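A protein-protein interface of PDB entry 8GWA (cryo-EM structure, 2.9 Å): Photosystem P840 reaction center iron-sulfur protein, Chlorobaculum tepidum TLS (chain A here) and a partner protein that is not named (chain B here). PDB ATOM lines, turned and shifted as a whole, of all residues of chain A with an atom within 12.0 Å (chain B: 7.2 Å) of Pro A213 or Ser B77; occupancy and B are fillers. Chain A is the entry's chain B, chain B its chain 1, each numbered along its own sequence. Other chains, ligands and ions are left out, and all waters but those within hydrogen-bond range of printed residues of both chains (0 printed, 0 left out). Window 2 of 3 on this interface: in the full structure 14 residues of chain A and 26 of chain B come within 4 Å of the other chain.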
ATOM      1  N   LEU A 206       0.841 -17.522  28.263  1.00  0.00           N
ATOM      2  CA  LEU A 206       1.723 -18.605  28.659  1.00  0.00           C
ATOM      3  C   LEU A 206       1.400 -19.852  27.845  1.00  0.00           C
ATOM      4  O   LEU A 206       0.451 -19.889  27.063  1.00  0.00           O
ATOM      5  CB  LEU A 206       1.586 -18.898  30.152  1.00  0.00           C
ATOM      6  CG  LEU A 206       2.244 -17.942  31.145  1.00  0.00           C
ATOM      7  CD1 LEU A 206       1.787 -18.271  32.556  1.00  0.00           C
ATOM      8  CD2 LEU A 206       3.752 -18.017  31.041  1.00  0.00           C
ATOM      9  N   PHE A 208       3.038 -23.164  29.394  1.00  0.00           N
ATOM     10  CA  PHE A 208       3.286 -24.166  30.414  1.00  0.00           C
ATOM     11  C   PHE A 208       3.879 -23.411  31.594  1.00  0.00           C
ATOM     12  O   PHE A 208       4.481 -22.348  31.421  1.00  0.00           O
ATOM     13  CB  PHE A 208       4.217 -25.266  29.883  1.00  0.00           C
ATOM     14  CG  PHE A 208       4.375 -26.442  30.803  1.00  0.00           C
ATOM     15  CD1 PHE A 208       3.375 -27.394  30.899  1.00  0.00           C
ATOM     16  CD2 PHE A 208       5.526 -26.614  31.547  1.00  0.00           C
ATOM     17  CE1 PHE A 208       3.515 -28.485  31.729  1.00  0.00           C
ATOM     18  CE2 PHE A 208       5.673 -27.702  32.382  1.00  0.00           C
ATOM     19  CZ  PHE A 208       4.667 -28.639  32.471  1.00  0.00           C
ATOM     20  N   SER A 209       3.690 -23.952  32.802  1.00  0.00           N
ATOM     21  CA  SER A 209       3.969 -23.164  34.001  1.00  0.00           C
ATOM     22  C   SER A 209       5.418 -22.698  34.042  1.00  0.00           C
ATOM     23  O   SER A 209       5.695 -21.544  34.396  1.00  0.00           O
ATOM     24  CB  SER A 209       3.626 -23.963  35.255  1.00  0.00           C
ATOM     25  OG  SER A 209       2.234 -23.922  35.516  1.00  0.00           O
ATOM     26  N   TYR A 210       6.358 -23.570  33.688  1.00  0.00           N
ATOM     27  CA  TYR A 210       7.741 -23.158  33.509  1.00  0.00           C
ATOM     28  C   TYR A 210       8.283 -23.780  32.231  1.00  0.00           C
ATOM     29  O   TYR A 210       7.968 -24.924  31.898  1.00  0.00           O
ATOM     30  CB  TYR A 210       8.630 -23.552  34.697  1.00  0.00           C
ATOM     31  CG  TYR A 210      10.100 -23.378  34.397  1.00  0.00           C
ATOM     32  CD1 TYR A 210      10.681 -22.119  34.419  1.00  0.00           C
ATOM     33  CD2 TYR A 210      10.899 -24.464  34.066  1.00  0.00           C
ATOM     34  CE1 TYR A 210      12.018 -21.944  34.132  1.00  0.00           C
ATOM     35  CE2 TYR A 210      12.240 -24.298  33.776  1.00  0.00           C
ATOM     36  CZ  TYR A 210      12.793 -23.035  33.812  1.00  0.00           C
ATOM     37  OH  TYR A 210      14.126 -22.859  33.525  1.00  0.00           O
ATOM     38  N   THR A 211       9.117 -23.020  31.525  1.00  0.00           N
ATOM     39  CA  THR A 211       9.703 -23.455  30.272  1.00  0.00           C
ATOM     40  C   THR A 211      11.219 -23.527  30.402  1.00  0.00           C
ATOM     41  O   THR A 211      11.829 -22.613  30.976  1.00  0.00           O
ATOM     42  CB  THR A 211       9.320 -22.500  29.131  1.00  0.00           C
ATOM     43  OG1 THR A 211       7.901 -22.307  29.127  1.00  0.00           O
ATOM     44  CG2 THR A 211       9.752 -23.064  27.789  1.00  0.00           C
ATOM     45  N   PRO A 212      11.855 -24.589  29.912  1.00  0.00           N
ATOM     46  CA  PRO A 212      13.320 -24.688  29.970  1.00  0.00           C
ATOM     47  C   PRO A 212      13.989 -23.490  29.317  1.00  0.00           C
ATOM     48  O   PRO A 212      13.368 -22.778  28.512  1.00  0.00           O
ATOM     49  CB  PRO A 212      13.604 -25.984  29.198  1.00  0.00           C
ATOM     50  CG  PRO A 212      12.409 -26.822  29.463  1.00  0.00           C
ATOM     51  CD  PRO A 212      11.233 -25.875  29.550  1.00  0.00           C
ATOM     52  N   PRO A 213      15.264 -23.236  29.631  1.00  0.00           N
ATOM     53  CA  PRO A 213      15.860 -21.928  29.320  1.00  0.00           C
ATOM     54  C   PRO A 213      16.392 -21.744  27.904  1.00  0.00           C
ATOM     55  O   PRO A 213      17.172 -20.813  27.682  1.00  0.00           O
ATOM     56  CB  PRO A 213      17.000 -21.824  30.340  1.00  0.00           C
ATOM     57  CG  PRO A 213      17.374 -23.229  30.626  1.00  0.00           C
ATOM     58  CD  PRO A 213      16.115 -24.031  30.536  1.00  0.00           C
ATOM     59  N   GLU A 214      16.019 -22.601  26.949  1.00  0.00           N
ATOM     60  CA  GLU A 214      16.376 -22.406  25.538  1.00  0.00           C
ATOM     61  C   GLU A 214      17.894 -22.329  25.350  1.00  0.00           C
ATOM     62  O   GLU A 214      18.443 -21.312  24.928  1.00  0.00           O
ATOM     63  CB  GLU A 214      15.704 -21.148  24.972  1.00  0.00           C
ATOM     64  CG  GLU A 214      14.191 -21.194  24.812  1.00  0.00           C
ATOM     65  CD  GLU A 214      13.741 -22.159  23.736  1.00  0.00           C
ATOM     66  OE1 GLU A 214      14.491 -22.348  22.756  1.00  0.00           O
ATOM     67  OE2 GLU A 214      12.622 -22.699  23.848  1.00  0.00           O
ATOM     68  N   ARG A 215      18.570 -23.428  25.666  1.00  0.00           N
ATOM     69  CA  ARG A 215      20.024 -23.436  25.719  1.00  0.00           C
ATOM     70  C   ARG A 215      20.647 -23.803  24.377  1.00  0.00           C
ATOM     71  O   ARG A 215      20.118 -24.626  23.625  1.00  0.00           O
ATOM     72  CB  ARG A 215      20.517 -24.420  26.780  1.00  0.00           C
ATOM     73  CG  ARG A 215      19.720 -24.435  28.066  1.00  0.00           C
ATOM     74  CD  ARG A 215      20.577 -24.985  29.192  1.00  0.00           C
ATOM     75  NE  ARG A 215      21.955 -24.523  29.071  1.00  0.00           N
ATOM     76  CZ  ARG A 215      22.999 -25.117  29.631  1.00  0.00           C
ATOM     77  NH1 ARG A 215      22.863 -26.205  30.371  1.00  0.00           N
ATOM     78  NH2 ARG A 215      24.212 -24.606  29.443  1.00  0.00           N
ATOM     79  N   LEU A 216      21.785 -23.176  24.082  1.00  0.00           N
ATOM     80  CA  LEU A 216      22.654 -23.662  23.020  1.00  0.00           C
ATOM     81  C   LEU A 216      23.318 -24.960  23.455  1.00  0.00           C
ATOM     82  O   LEU A 216      23.773 -25.099  24.594  1.00  0.00           O
ATOM     83  CB  LEU A 216      23.733 -22.634  22.678  1.00  0.00           C
ATOM     84  CG  LEU A 216      23.370 -21.347  21.944  1.00  0.00           C
ATOM     85  CD1 LEU A 216      24.605 -20.479  21.789  1.00  0.00           C
ATOM     86  CD2 LEU A 216      22.757 -21.654  20.590  1.00  0.00           C
ATOM     87  N   ASP A 217      23.384 -25.917  22.534  1.00  0.00           N
ATOM     88  CA  ASP A 217      23.867 -27.248  22.864  1.00  0.00           C
ATOM     89  C   ASP A 217      24.962 -27.666  21.895  1.00  0.00           C
ATOM     90  O   ASP A 217      24.986 -27.244  20.736  1.00  0.00           O
ATOM     91  CB  ASP A 217      22.733 -28.283  22.829  1.00  0.00           C
ATOM     92  CG  ASP A 217      21.671 -28.036  23.891  1.00  0.00           C
ATOM     93  OD1 ASP A 217      21.812 -27.091  24.691  1.00  0.00           O
ATOM     94  OD2 ASP A 217      20.680 -28.795  23.924  1.00  0.00           O
ATOM     95  N   LEU B  45      22.034 -17.257  34.404  1.00  0.00           N
ATOM     96  CA  LEU B  45      22.373 -18.595  33.954  1.00  0.00           C
ATOM     97  C   LEU B  45      21.125 -19.311  33.461  1.00  0.00           C
ATOM     98  O   LEU B  45      20.022 -19.050  33.951  1.00  0.00           O
ATOM     99  CB  LEU B  45      23.024 -19.405  35.084  1.00  0.00           C
ATOM    100  CG  LEU B  45      24.469 -19.016  35.398  1.00  0.00           C
ATOM    101  CD1 LEU B  45      24.985 -19.762  36.616  1.00  0.00           C
ATOM    102  CD2 LEU B  45      25.353 -19.265  34.192  1.00  0.00           C
ATOM    103  N   PRO B  46      21.267 -20.222  32.487  1.00  0.00           N
ATOM    104  CA  PRO B  46      22.518 -20.571  31.803  1.00  0.00           C
ATOM    105  C   PRO B  46      22.942 -19.526  30.779  1.00  0.00           C
ATOM    106  O   PRO B  46      22.096 -18.810  30.246  1.00  0.00           O
ATOM    107  CB  PRO B  46      22.184 -21.893  31.116  1.00  0.00           C
ATOM    108  CG  PRO B  46      20.724 -21.828  30.884  1.00  0.00           C
ATOM    109  CD  PRO B  46      20.137 -21.044  32.019  1.00  0.00           C
ATOM    110  N   ALA B  47      24.243 -19.445  30.507  1.00  0.00           N
ATOM    111  CA  ALA B  47      24.792 -18.484  29.559  1.00  0.00           C
ATOM    112  C   ALA B  47      25.651 -19.236  28.553  1.00  0.00           C
ATOM    113  O   ALA B  47      26.841 -19.457  28.791  1.00  0.00           O
ATOM    114  CB  ALA B  47      25.607 -17.408  30.276  1.00  0.00           C
ATOM    115  N   ASP B  48      25.062 -19.601  27.420  1.00  0.00           N
ATOM    116  CA  ASP B  48      25.746 -20.367  26.390  1.00  0.00           C
ATOM    117  C   ASP B  48      26.229 -19.427  25.298  1.00  0.00           C
ATOM    118  O   ASP B  48      25.559 -18.442  24.978  1.00  0.00           O
ATOM    119  CB  ASP B  48      24.825 -21.428  25.792  1.00  0.00           C
ATOM    120  CG  ASP B  48      24.463 -22.509  26.784  1.00  0.00           C
ATOM    121  OD1 ASP B  48      25.275 -22.785  27.689  1.00  0.00           O
ATOM    122  OD2 ASP B  48      23.365 -23.087  26.658  1.00  0.00           O
ATOM    123  N   SER B  73      25.112 -16.091  21.161  1.00  0.00           N
ATOM    124  CA  SER B  73      25.042 -16.516  22.549  1.00  0.00           C
ATOM    125  C   SER B  73      23.597 -16.521  23.019  1.00  0.00           C
ATOM    126  O   SER B  73      22.736 -15.840  22.457  1.00  0.00           O
ATOM    127  CB  SER B  73      25.879 -15.602  23.451  1.00  0.00           C
ATOM    128  OG  SER B  73      27.237 -15.597  23.053  1.00  0.00           O
ATOM    129  N   ILE B  74      23.334 -17.309  24.059  1.00  0.00           N
ATOM    130  CA  ILE B  74      22.054 -17.289  24.760  1.00  0.00           C
ATOM    131  C   ILE B  74      22.334 -17.194  26.251  1.00  0.00           C
ATOM    132  O   ILE B  74      23.062 -18.027  26.805  1.00  0.00           O
ATOM    133  CB  ILE B  74      21.190 -18.523  24.452  1.00  0.00           C
ATOM    134  CG1 ILE B  74      20.833 -18.574  22.968  1.00  0.00           C
ATOM    135  CG2 ILE B  74      19.928 -18.506  25.296  1.00  0.00           C
ATOM    136  CD1 ILE B  74      20.195 -19.873  22.540  1.00  0.00           C
ATOM    137  N   VAL B  75      21.760 -16.184  26.899  1.00  0.00           N
ATOM    138  CA  VAL B  75      21.898 -15.977  28.335  1.00  0.00           C
ATOM    139  C   VAL B  75      20.502 -15.810  28.914  1.00  0.00           C
ATOM    140  O   VAL B  75      19.807 -14.841  28.586  1.00  0.00           O
ATOM    141  CB  VAL B  75      22.769 -14.754  28.660  1.00  0.00           C
ATOM    142  CG1 VAL B  75      22.858 -14.551  30.158  1.00  0.00           C
ATOM    143  CG2 VAL B  75      24.152 -14.909  28.054  1.00  0.00           C
ATOM    144  N   ASP B  76      20.100 -16.737  29.782  1.00  0.00           N
ATOM    145  CA  ASP B  76      18.768 -16.735  30.388  1.00  0.00           C
ATOM    146  C   ASP B  76      17.680 -16.681  29.316  1.00  0.00           C
ATOM    147  O   ASP B  76      16.755 -15.867  29.368  1.00  0.00           O
ATOM    148  CB  ASP B  76      18.622 -15.584  31.386  1.00  0.00           C
ATOM    149  CG  ASP B  76      17.573 -15.861  32.448  1.00  0.00           C
ATOM    150  OD1 ASP B  76      16.381 -15.982  32.098  1.00  0.00           O
ATOM    151  OD2 ASP B  76      17.944 -15.964  33.636  1.00  0.00           O
ATOM    152  N   SER B  77      17.822 -17.554  28.316  1.00  0.00           N
ATOM    153  CA  SER B  77      16.862 -17.702  27.219  1.00  0.00           C
ATOM    154  C   SER B  77      16.774 -16.446  26.356  1.00  0.00           C
ATOM    155  O   SER B  77      15.782 -16.232  25.657  1.00  0.00           O
ATOM    156  CB  SER B  77      15.471 -18.091  27.734  1.00  0.00           C
ATOM    157  OG  SER B  77      14.855 -17.015  28.421  1.00  0.00           O
ATOM    158  N   THR B  78      17.807 -15.609  26.389  1.00  0.00           N
ATOM    159  CA  THR B  78      17.884 -14.417  25.550  1.00  0.00           C
ATOM    160  C   THR B  78      18.935 -14.673  24.480  1.00  0.00           C
ATOM    161  O   THR B  78      20.132 -14.726  24.777  1.00  0.00           O
ATOM    162  CB  THR B  78      18.227 -13.179  26.375  1.00  0.00           C
ATOM    163  OG1 THR B  78      17.173 -12.919  27.311  1.00  0.00           O
ATOM    164  CG2 THR B  78      18.397 -11.970  25.470  1.00  0.00           C
ATOM    165  N   LYS B  79      18.488 -14.822  23.235  1.00  0.00           N
ATOM    166  CA  LYS B  79      19.373 -15.188  22.133  1.00  0.00           C
ATOM    167  C   LYS B  79      20.132 -13.948  21.680  1.00  0.00           C
ATOM    168  O   LYS B  79      19.591 -13.091  20.980  1.00  0.00           O
ATOM    169  CB  LYS B  79      18.578 -15.802  20.987  1.00  0.00           C
ATOM    170  CG  LYS B  79      17.990 -17.164  21.306  1.00  0.00           C
ATOM    171  CD  LYS B  79      17.617 -17.921  20.045  1.00  0.00           C
ATOM    172  CE  LYS B  79      17.143 -19.329  20.368  1.00  0.00           C
ATOM    173  NZ  LYS B  79      16.856 -20.116  19.138  1.00  0.00           N
ATOM    174  N   ASN B  80      21.396 -13.856  22.078  1.00  0.00           N
ATOM    175  CA  ASN B  80      22.255 -12.739  21.719  1.00  0.00           C
ATOM    176  C   ASN B  80      23.122 -13.110  20.524  1.00  0.00           C
ATOM    177  O   ASN B  80      23.529 -14.263  20.361  1.00  0.00           O
ATOM    178  CB  ASN B  80      23.143 -12.338  22.898  1.00  0.00           C
ATOM    179  CG  ASN B  80      22.347 -12.008  24.142  1.00  0.00           C
ATOM    180  OD1 ASN B  80      21.327 -11.323  24.076  1.00  0.00           O
ATOM    181  ND2 ASN B  80      22.808 -12.496  25.286  1.00  0.00           N
ATOM    182  N   GLY B 107      17.580 -10.715  21.199  1.00  0.00           N
ATOM    183  CA  GLY B 107      16.147 -10.953  21.174  1.00  0.00           C
ATOM    184  C   GLY B 107      15.550 -10.399  19.897  1.00  0.00           C
ATOM    185  O   GLY B 107      15.951 -10.763  18.784  1.00  0.00           O
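Among the printed residues, pairs that only touch across the chains: Glu A214 with Ile B74 (3.2 Å), Arg A215 with Pro B46 (3.3 Å), Leu A216 with Ile B74 (3.6 Å) and Pro A213 with Pro B46 (3.6 Å).
O of Pro B46 sits at hydrogen-bond distance from N of Asp B76 (2.9 Å).
N of Asp B48 is in hydrogen-bond range of O of Ile B74, 2.6 Å away.
Of the 13 printed residues of chain B, 4 touch a printed residue of chain A.
Printed residues of chain B that touch a printed residue of chain A: Pro B46, Asp B48, Ile B74 and Ser B77.
Hydrophobic or aromatic side chains of chain A that line the printed part of chain B: Pro A213 and Leu A216.
Along chain A the printed residues that touch a printed residue of chain B span positions 213 to 216.
Among the printed residues, Asp or Glu carboxylates within 4 Å of a Lys or Arg side-chain nitrogen of the other chain: Arg A215 with Asp B48 (2.7 Å).
Pro A213 touches two residues of chain B.
Of the printed residues of chain A, Ser B77 touches Pro A213.
Pro B46 touches two residues of chain A.
No residue of chain A comes within 4 Å of Asp B76.
No residue of chain A comes within 4 Å of Thr B78.
No residue of chain A comes within 4 Å of Lys B79.
Printed residues of chain A within 4 Å of Asp B48: Arg A215 (2.7 Å) and Leu A216 (2.9 Å).
Of the printed residues of chain B, Leu A216 touches Asp B48 and Ile B74.
Asp A217 touches none of the printed residues of chain B.
The nearest residue of chain B that does not touch Pro A213 is Ile B74 (4.3 Å).
The side-chain carboxylate (OD1) of Asp B48 is in salt-bridge range of the guanidinium group (NH2) of Arg A215.
N of Leu A216 is in hydrogen-bond range of OD2 of Asp B48 (3.0 Å).
N of Ser B77 sits close to O of Pro A213 (3.4 Å).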
